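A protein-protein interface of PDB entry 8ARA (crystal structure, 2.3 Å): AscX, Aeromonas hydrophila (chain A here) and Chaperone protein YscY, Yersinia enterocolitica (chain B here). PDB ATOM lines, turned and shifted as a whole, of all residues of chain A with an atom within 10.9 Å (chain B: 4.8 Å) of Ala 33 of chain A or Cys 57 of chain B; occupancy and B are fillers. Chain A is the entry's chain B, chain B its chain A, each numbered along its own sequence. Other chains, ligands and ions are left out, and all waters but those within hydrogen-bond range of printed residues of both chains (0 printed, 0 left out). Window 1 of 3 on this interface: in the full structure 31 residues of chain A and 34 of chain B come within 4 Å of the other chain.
Printed residues of chain B that touch a printed residue of chain A: Leu 22, Trp 26, Leu 29, Arg 56, Cys 57 and Val 60.
Hydrophobic or aromatic side chains of chain A that line the printed part of chain B: Phe 32, Ala 33 and Pro 35.
Among the printed residues, 10 pairs touch across the chains.
The side-chain hydroxyl (OG1) of Thr 34 of chain A lies within hydrogen-bond range of the backbone carbonyl oxygen (O) of Leu 30 of chain A, at 2.7 Å.
The backbone carbonyl oxygen (O) of Leu 88 of chain A lies within hydrogen-bond range of the backbone NH (N) of Lys 93 of chain A (3.0 Å).
SG of Cys 57 of chain B sits at hydrogen-bond distance from O of Ala 33 of chain A.
Among the printed residues, merely in contact across the chains: Leu 29 of chain A with Val 60 of chain B (3.3 Å), Thr 34 of chain A with Trp 26 of chain B (3.5 Å), Pro 35 of chain A with Trp 26 of chain B (3.5 Å), Lys 93 of chain A with Trp 26 of chain B (3.5 Å), Phe 32 of chain A with Arg 56 of chain B (3.6 Å), Ala 33 of chain A with Val 60 of chain B (3.6 Å), Ala 33 of chain A with Trp 26 of chain B (3.7 Å), Ala 33 of chain A with Leu 29 of chain B (3.7 Å) and Pro 35 of chain A with Leu 22 of chain B (3.7 Å).
Of the printed residues of chain B, Ala 33 of chain A touches Trp 26, Leu 29, Cys 57 and Val 60.
No residue of chain A comes within 4 Å of Gly 25 of chain B.
No residue of chain A comes within 4 Å of Ala 53 of chain B.
No residue of chain A comes within 4 Å of Ala 61 of chain B.
Of the printed residues of chain A, Val 60 of chain B touches Leu 29 and Ala 33.
Of the printed residues of chain A, Leu 29 of chain B touches Ala 33 (3.7 Å).
The nearest residue of chain B that does not touch Ala 33 of chain A is Arg 56 of chain B (4.1 Å).
The nearest residue of chain A that does not touch Cys 57 of chain B is Pro 35 of chain A (5.1 Å).
The nearest printed residue of chain A that does not touch Leu 22 of chain B is Ala 33 of chain A (6.0 Å).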
ATOM      1  N   ALA A  25      -5.750 -23.708  -6.957  1.00  0.00           N
ATOM      2  CA  ALA A  25      -6.258 -24.800  -7.782  1.00  0.00           C
ATOM      3  C   ALA A  25      -7.107 -24.281  -8.934  1.00  0.00           C
ATOM      4  O   ALA A  25      -6.957 -24.735 -10.073  1.00  0.00           O
ATOM      5  CB  ALA A  25      -7.065 -25.774  -6.927  1.00  0.00           C
ATOM      6  N   ASP A  26      -8.017 -23.345  -8.656  1.00  0.00           N
ATOM      7  CA  ASP A  26      -8.877 -22.826  -9.713  1.00  0.00           C
ATOM      8  C   ASP A  26      -8.058 -22.114 -10.779  1.00  0.00           C
ATOM      9  O   ASP A  26      -8.285 -22.310 -11.978  1.00  0.00           O
ATOM     10  CB  ASP A  26      -9.928 -21.884  -9.125  1.00  0.00           C
ATOM     11  CG  ASP A  26     -10.794 -22.554  -8.078  1.00  0.00           C
ATOM     12  OD1 ASP A  26     -10.361 -23.580  -7.510  1.00  0.00           O
ATOM     13  OD2 ASP A  26     -11.912 -22.055  -7.827  1.00  0.00           O
ATOM     14  N   ARG A  27      -7.097 -21.289 -10.361  1.00  0.00           N
ATOM     15  CA  ARG A  27      -6.248 -20.595 -11.321  1.00  0.00           C
ATOM     16  C   ARG A  27      -5.438 -21.580 -12.153  1.00  0.00           C
ATOM     17  O   ARG A  27      -5.215 -21.348 -13.346  1.00  0.00           O
ATOM     18  CB  ARG A  27      -5.330 -19.616 -10.588  1.00  0.00           C
ATOM     19  CG  ARG A  27      -4.407 -18.811 -11.492  1.00  0.00           C
ATOM     20  CD  ARG A  27      -5.203 -18.040 -12.528  1.00  0.00           C
ATOM     21  NE  ARG A  27      -4.362 -17.270 -13.438  1.00  0.00           N
ATOM     22  CZ  ARG A  27      -4.215 -15.953 -13.386  1.00  0.00           C
ATOM     23  NH1 ARG A  27      -4.832 -15.223 -12.471  1.00  0.00           N
ATOM     24  NH2 ARG A  27      -3.434 -15.351 -14.281  1.00  0.00           N
ATOM     25  N   ALA A  28      -5.014 -22.694 -11.554  1.00  0.00           N
ATOM     26  CA  ALA A  28      -4.232 -23.680 -12.293  1.00  0.00           C
ATOM     27  C   ALA A  28      -5.090 -24.427 -13.304  1.00  0.00           C
ATOM     28  O   ALA A  28      -4.612 -24.785 -14.386  1.00  0.00           O
ATOM     29  CB  ALA A  28      -3.569 -24.659 -11.327  1.00  0.00           C
ATOM     30  N   LEU A  29      -6.356 -24.686 -12.968  1.00  0.00           N
ATOM     31  CA  LEU A  29      -7.234 -25.385 -13.901  1.00  0.00           C
ATOM     32  C   LEU A  29      -7.503 -24.545 -15.142  1.00  0.00           C
ATOM     33  O   LEU A  29      -7.518 -25.071 -16.261  1.00  0.00           O
ATOM     34  CB  LEU A  29      -8.548 -25.759 -13.213  1.00  0.00           C
ATOM     35  CG  LEU A  29      -8.537 -26.931 -12.230  1.00  0.00           C
ATOM     36  CD1 LEU A  29      -9.831 -26.961 -11.439  1.00  0.00           C
ATOM     37  CD2 LEU A  29      -8.337 -28.242 -12.968  1.00  0.00           C
ATOM     38  N   LEU A  30      -7.706 -23.237 -14.967  1.00  0.00           N
ATOM     39  CA  LEU A  30      -8.033 -22.379 -16.098  1.00  0.00           C
ATOM     40  C   LEU A  30      -6.805 -22.024 -16.926  1.00  0.00           C
ATOM     41  O   LEU A  30      -6.932 -21.766 -18.127  1.00  0.00           O
ATOM     42  CB  LEU A  30      -8.742 -21.120 -15.605  1.00  0.00           C
ATOM     43  CG  LEU A  30     -10.193 -21.357 -15.176  1.00  0.00           C
ATOM     44  CD1 LEU A  30     -10.584 -20.510 -13.977  1.00  0.00           C
ATOM     45  CD2 LEU A  30     -11.125 -21.087 -16.342  1.00  0.00           C
ATOM     46  N   ASP A  31      -5.619 -21.997 -16.313  1.00  0.00           N
ATOM     47  CA  ASP A  31      -4.394 -21.941 -17.106  1.00  0.00           C
ATOM     48  C   ASP A  31      -4.217 -23.220 -17.914  1.00  0.00           C
ATOM     49  O   ASP A  31      -3.826 -23.173 -19.086  1.00  0.00           O
ATOM     50  CB  ASP A  31      -3.183 -21.712 -16.201  1.00  0.00           C
ATOM     51  CG  ASP A  31      -3.195 -20.349 -15.537  1.00  0.00           C
ATOM     52  OD1 ASP A  31      -3.794 -19.412 -16.105  1.00  0.00           O
ATOM     53  OD2 ASP A  31      -2.600 -20.215 -14.447  1.00  0.00           O
ATOM     54  N   PHE A  32      -4.510 -24.366 -17.296  1.00  0.00           N
ATOM     55  CA  PHE A  32      -4.420 -25.654 -17.978  1.00  0.00           C
ATOM     56  C   PHE A  32      -5.314 -25.693 -19.213  1.00  0.00           C
ATOM     57  O   PHE A  32      -4.934 -26.253 -20.248  1.00  0.00           O
ATOM     58  CB  PHE A  32      -4.789 -26.764 -16.990  1.00  0.00           C
ATOM     59  CG  PHE A  32      -4.719 -28.154 -17.556  1.00  0.00           C
ATOM     60  CD1 PHE A  32      -3.499 -28.777 -17.757  1.00  0.00           C
ATOM     61  CD2 PHE A  32      -5.877 -28.854 -17.849  1.00  0.00           C
ATOM     62  CE1 PHE A  32      -3.438 -30.059 -18.265  1.00  0.00           C
ATOM     63  CE2 PHE A  32      -5.820 -30.139 -18.355  1.00  0.00           C
ATOM     64  CZ  PHE A  32      -4.601 -30.740 -18.562  1.00  0.00           C
ATOM     65  N   ALA A  33      -6.498 -25.086 -19.134  1.00  0.00           N
ATOM     66  CA  ALA A  33      -7.423 -25.080 -20.258  1.00  0.00           C
ATOM     67  C   ALA A  33      -7.061 -24.061 -21.330  1.00  0.00           C
ATOM     68  O   ALA A  33      -7.596 -24.141 -22.442  1.00  0.00           O
ATOM     69  CB  ALA A  33      -8.845 -24.810 -19.766  1.00  0.00           C
ATOM     70  N   THR A  34      -6.182 -23.114 -21.026  1.00  0.00           N
ATOM     71  CA  THR A  34      -5.861 -22.046 -21.965  1.00  0.00           C
ATOM     72  C   THR A  34      -5.035 -22.589 -23.123  1.00  0.00           C
ATOM     73  O   THR A  34      -3.945 -23.128 -22.894  1.00  0.00           O
ATOM     74  CB  THR A  34      -5.099 -20.930 -21.259  1.00  0.00           C
ATOM     75  OG1 THR A  34      -5.900 -20.397 -20.199  1.00  0.00           O
ATOM     76  CG2 THR A  34      -4.763 -19.818 -22.238  1.00  0.00           C
ATOM     77  N   PRO A  35      -5.500 -22.477 -24.364  1.00  0.00           N
ATOM     78  CA  PRO A  35      -4.691 -22.929 -25.499  1.00  0.00           C
ATOM     79  C   PRO A  35      -3.552 -21.967 -25.801  1.00  0.00           C
ATOM     80  O   PRO A  35      -3.642 -20.760 -25.566  1.00  0.00           O
ATOM     81  CB  PRO A  35      -5.697 -22.967 -26.655  1.00  0.00           C
ATOM     82  CG  PRO A  35      -6.709 -21.939 -26.290  1.00  0.00           C
ATOM     83  CD  PRO A  35      -6.828 -21.997 -24.786  1.00  0.00           C
ATOM     84  N   HIS A  36      -2.469 -22.528 -26.332  1.00  0.00           N
ATOM     85  CA  HIS A  36      -1.292 -21.743 -26.692  1.00  0.00           C
ATOM     86  C   HIS A  36      -1.273 -21.417 -28.186  1.00  0.00           C
ATOM     87  O   HIS A  36      -1.206 -20.251 -28.582  1.00  0.00           O
ATOM     88  CB  HIS A  36      -0.016 -22.493 -26.302  1.00  0.00           C
ATOM     89  CG  HIS A  36       0.049 -22.857 -24.851  1.00  0.00           C
ATOM     90  ND1 HIS A  36      -0.699 -22.216 -23.886  1.00  0.00           N
ATOM     91  CD2 HIS A  36       0.771 -23.800 -24.200  1.00  0.00           C
ATOM     92  CE1 HIS A  36      -0.440 -22.747 -22.704  1.00  0.00           C
ATOM     93  NE2 HIS A  36       0.449 -23.711 -22.867  1.00  0.00           N
ATOM     94  N   LEU A  88     -12.346 -11.528 -27.644  1.00  0.00           N
ATOM     95  CA  LEU A  88     -11.143 -12.274 -27.994  1.00  0.00           C
ATOM     96  C   LEU A  88      -9.991 -11.343 -28.332  1.00  0.00           C
ATOM     97  O   LEU A  88      -8.831 -11.659 -28.047  1.00  0.00           O
ATOM     98  CB  LEU A  88     -11.423 -13.208 -29.167  1.00  0.00           C
ATOM     99  CG  LEU A  88     -12.010 -14.580 -28.839  1.00  0.00           C
ATOM    100  CD1 LEU A  88     -12.407 -15.296 -30.116  1.00  0.00           C
ATOM    101  CD2 LEU A  88     -11.010 -15.416 -28.052  1.00  0.00           C
ATOM    102  N   LYS A  93      -6.037 -12.782 -28.155  1.00  0.00           N
ATOM    103  CA  LYS A  93      -6.112 -14.097 -28.783  1.00  0.00           C
ATOM    104  C   LYS A  93      -6.449 -14.041 -30.265  1.00  0.00           C
ATOM    105  O   LYS A  93      -5.876 -14.804 -31.049  1.00  0.00           O
ATOM    106  CB  LYS A  93      -7.145 -14.971 -28.054  1.00  0.00           C
ATOM    107  CG  LYS A  93      -6.854 -15.178 -26.575  1.00  0.00           C
ATOM    108  CD  LYS A  93      -5.548 -15.928 -26.362  1.00  0.00           C
ATOM    109  CE  LYS A  93      -5.274 -16.148 -24.879  1.00  0.00           C
ATOM    110  NZ  LYS A  93      -3.988 -16.865 -24.647  1.00  0.00           N
ATOM    111  N   LEU B  22     -11.485 -23.978 -31.520  1.00  0.00           N
ATOM    112  CA  LEU B  22     -10.933 -24.128 -30.178  1.00  0.00           C
ATOM    113  C   LEU B  22     -10.942 -22.807 -29.415  1.00  0.00           C
ATOM    114  O   LEU B  22     -11.248 -22.779 -28.217  1.00  0.00           O
ATOM    115  CB  LEU B  22      -9.513 -24.690 -30.263  1.00  0.00           C
ATOM    116  CG  LEU B  22      -8.669 -24.681 -28.984  1.00  0.00           C
ATOM    117  CD1 LEU B  22      -9.243 -25.643 -27.960  1.00  0.00           C
ATOM    118  CD2 LEU B  22      -7.226 -25.027 -29.306  1.00  0.00           C
ATOM    119  N   GLY B  25     -14.390 -22.066 -28.263  1.00  0.00           N
ATOM    120  CA  GLY B  25     -14.723 -22.900 -27.123  1.00  0.00           C
ATOM    121  C   GLY B  25     -14.079 -22.403 -25.846  1.00  0.00           C
ATOM    122  O   GLY B  25     -14.699 -22.419 -24.778  1.00  0.00           O
ATOM    123  N   TRP B  26     -12.827 -21.949 -25.935  1.00  0.00           N
ATOM    124  CA  TRP B  26     -12.169 -21.384 -24.763  1.00  0.00           C
ATOM    125  C   TRP B  26     -12.792 -20.049 -24.369  1.00  0.00           C
ATOM    126  O   TRP B  26     -12.939 -19.755 -23.176  1.00  0.00           O
ATOM    127  CB  TRP B  26     -10.674 -21.229 -25.028  1.00  0.00           C
ATOM    128  CG  TRP B  26      -9.950 -20.523 -23.925  1.00  0.00           C
ATOM    129  CD1 TRP B  26      -9.541 -21.056 -22.738  1.00  0.00           C
ATOM    130  CD2 TRP B  26      -9.551 -19.149 -23.907  1.00  0.00           C
ATOM    131  NE1 TRP B  26      -8.909 -20.097 -21.981  1.00  0.00           N
ATOM    132  CE2 TRP B  26      -8.902 -18.918 -22.678  1.00  0.00           C
ATOM    133  CE3 TRP B  26      -9.682 -18.090 -24.812  1.00  0.00           C
ATOM    134  CZ2 TRP B  26      -8.383 -17.672 -22.330  1.00  0.00           C
ATOM    135  CZ3 TRP B  26      -9.165 -16.856 -24.467  1.00  0.00           C
ATOM    136  CH2 TRP B  26      -8.525 -16.656 -23.235  1.00  0.00           C
ATOM    137  N   LEU B  29     -15.700 -20.668 -22.268  1.00  0.00           N
ATOM    138  CA  LEU B  29     -15.250 -21.113 -20.954  1.00  0.00           C
ATOM    139  C   LEU B  29     -14.738 -19.941 -20.130  1.00  0.00           C
ATOM    140  O   LEU B  29     -15.195 -19.709 -19.004  1.00  0.00           O
ATOM    141  CB  LEU B  29     -14.159 -22.170 -21.105  1.00  0.00           C
ATOM    142  CG  LEU B  29     -13.454 -22.526 -19.801  1.00  0.00           C
ATOM    143  CD1 LEU B  29     -14.413 -23.275 -18.904  1.00  0.00           C
ATOM    144  CD2 LEU B  29     -12.207 -23.344 -20.062  1.00  0.00           C
ATOM    145  N   LEU B  41     -16.612 -27.667 -28.151  1.00  0.00           N
ATOM    146  CA  LEU B  41     -15.444 -28.534 -28.097  1.00  0.00           C
ATOM    147  C   LEU B  41     -15.785 -30.002 -28.327  1.00  0.00           C
ATOM    148  O   LEU B  41     -14.915 -30.760 -28.769  1.00  0.00           O
ATOM    149  CB  LEU B  41     -14.734 -28.346 -26.758  1.00  0.00           C
ATOM    150  CG  LEU B  41     -14.116 -26.950 -26.606  1.00  0.00           C
ATOM    151  CD1 LEU B  41     -13.796 -26.643 -25.159  1.00  0.00           C
ATOM    152  CD2 LEU B  41     -12.866 -26.835 -27.471  1.00  0.00           C
ATOM    153  N   ALA B  53      -5.142 -29.840 -26.965  1.00  0.00           N
ATOM    154  CA  ALA B  53      -5.579 -28.556 -26.422  1.00  0.00           C
ATOM    155  C   ALA B  53      -7.096 -28.487 -26.298  1.00  0.00           C
ATOM    156  O   ALA B  53      -7.614 -27.865 -25.365  1.00  0.00           O
ATOM    157  CB  ALA B  53      -5.059 -27.409 -27.286  1.00  0.00           C
ATOM    158  N   GLY B  54      -7.822 -29.125 -27.218  1.00  0.00           N
ATOM    159  CA  GLY B  54      -9.264 -29.217 -27.073  1.00  0.00           C
ATOM    160  C   GLY B  54      -9.686 -30.190 -25.994  1.00  0.00           C
ATOM    161  O   GLY B  54     -10.684 -29.963 -25.304  1.00  0.00           O
ATOM    162  N   ARG B  55      -8.945 -31.292 -25.840  1.00  0.00           N
ATOM    163  CA  ARG B  55      -9.204 -32.210 -24.738  1.00  0.00           C
ATOM    164  C   ARG B  55      -9.066 -31.503 -23.397  1.00  0.00           C
ATOM    165  O   ARG B  55      -9.913 -31.668 -22.512  1.00  0.00           O
ATOM    166  CB  ARG B  55      -8.249 -33.400 -24.814  1.00  0.00           C
ATOM    167  CG  ARG B  55      -8.564 -34.389 -25.913  1.00  0.00           C
ATOM    168  CD  ARG B  55      -9.658 -35.348 -25.489  1.00  0.00           C
ATOM    169  NE  ARG B  55      -9.839 -36.419 -26.460  1.00  0.00           N
ATOM    170  CZ  ARG B  55     -10.634 -37.464 -26.280  1.00  0.00           C
ATOM    171  NH1 ARG B  55     -11.337 -37.616 -25.168  1.00  0.00           N
ATOM    172  NH2 ARG B  55     -10.727 -38.382 -27.240  1.00  0.00           N
ATOM    173  N   ARG B  56      -8.005 -30.704 -23.231  1.00  0.00           N
ATOM    174  CA  ARG B  56      -7.793 -30.005 -21.966  1.00  0.00           C
ATOM    175  C   ARG B  56      -8.858 -28.943 -21.738  1.00  0.00           C
ATOM    176  O   ARG B  56      -9.343 -28.772 -20.614  1.00  0.00           O
ATOM    177  CB  ARG B  56      -6.404 -29.365 -21.927  1.00  0.00           C
ATOM    178  CG  ARG B  56      -5.242 -30.306 -22.179  1.00  0.00           C
ATOM    179  CD  ARG B  56      -3.913 -29.610 -21.900  1.00  0.00           C
ATOM    180  NE  ARG B  56      -2.821 -30.177 -22.683  1.00  0.00           N
ATOM    181  CZ  ARG B  56      -2.153 -31.275 -22.357  1.00  0.00           C
ATOM    182  NH1 ARG B  56      -2.432 -31.956 -21.255  1.00  0.00           N
ATOM    183  NH2 ARG B  56      -1.183 -31.706 -23.160  1.00  0.00           N
ATOM    184  N   CYS B  57      -9.227 -28.212 -22.787  1.00  0.00           N
ATOM    185  CA  CYS B  57     -10.223 -27.163 -22.618  1.00  0.00           C
ATOM    186  C   CYS B  57     -11.592 -27.756 -22.303  1.00  0.00           C
ATOM    187  O   CYS B  57     -12.279 -27.285 -21.389  1.00  0.00           O
ATOM    188  CB  CYS B  57     -10.276 -26.282 -23.867  1.00  0.00           C
ATOM    189  SG  CYS B  57     -11.034 -24.666 -23.582  1.00  0.00           S
ATOM    190  N   ARG B  58     -11.998 -28.800 -23.033  1.00  0.00           N
ATOM    191  CA  ARG B  58     -13.284 -29.432 -22.752  1.00  0.00           C
ATOM    192  C   ARG B  58     -13.306 -30.037 -21.353  1.00  0.00           C
ATOM    193  O   ARG B  58     -14.338 -30.009 -20.670  1.00  0.00           O
ATOM    194  CB  ARG B  58     -13.600 -30.502 -23.800  1.00  0.00           C
ATOM    195  CG  ARG B  58     -14.913 -31.224 -23.512  1.00  0.00           C
ATOM    196  CD  ARG B  58     -15.279 -32.232 -24.574  1.00  0.00           C
ATOM    197  NE  ARG B  58     -14.446 -33.427 -24.525  1.00  0.00           N
ATOM    198  CZ  ARG B  58     -14.661 -34.509 -25.261  1.00  0.00           C
ATOM    199  NH1 ARG B  58     -15.695 -34.592 -26.080  1.00  0.00           N
ATOM    200  NH2 ARG B  58     -13.810 -35.529 -25.180  1.00  0.00           N
ATOM    201  N   LEU B  59     -12.175 -30.587 -20.911  1.00  0.00           N
ATOM    202  CA  LEU B  59     -12.098 -31.157 -19.571  1.00  0.00           C
ATOM    203  C   LEU B  59     -12.443 -30.117 -18.513  1.00  0.00           C
ATOM    204  O   LEU B  59     -13.329 -30.334 -17.679  1.00  0.00           O
ATOM    205  CB  LEU B  59     -10.701 -31.731 -19.339  1.00  0.00           C
ATOM    206  CG  LEU B  59     -10.382 -32.377 -17.993  1.00  0.00           C
ATOM    207  CD1 LEU B  59     -11.540 -33.229 -17.489  1.00  0.00           C
ATOM    208  CD2 LEU B  59      -9.136 -33.217 -18.155  1.00  0.00           C
ATOM    209  N   VAL B  60     -11.754 -28.976 -18.532  1.00  0.00           N
ATOM    210  CA  VAL B  60     -12.050 -27.928 -17.563  1.00  0.00           C
ATOM    211  C   VAL B  60     -13.443 -27.360 -17.801  1.00  0.00           C
ATOM    212  O   VAL B  60     -14.122 -26.945 -16.856  1.00  0.00           O
ATOM    213  CB  VAL B  60     -10.963 -26.839 -17.616  1.00  0.00           C
ATOM    214  CG1 VAL B  60     -11.255 -25.729 -16.614  1.00  0.00           C
ATOM    215  CG2 VAL B  60      -9.599 -27.458 -17.352  1.00  0.00           C
ATOM    216  N   ALA B  61     -13.900 -27.345 -19.054  1.00  0.00           N
ATOM    217  CA  ALA B  61     -15.266 -26.920 -19.334  1.00  0.00           C
ATOM    218  C   ALA B  61     -16.277 -27.863 -18.692  1.00  0.00           C
ATOM    219  O   ALA B  61     -17.278 -27.417 -18.120  1.00  0.00           O
ATOM    220  CB  ALA B  61     -15.485 -26.836 -20.842  1.00  0.00           C
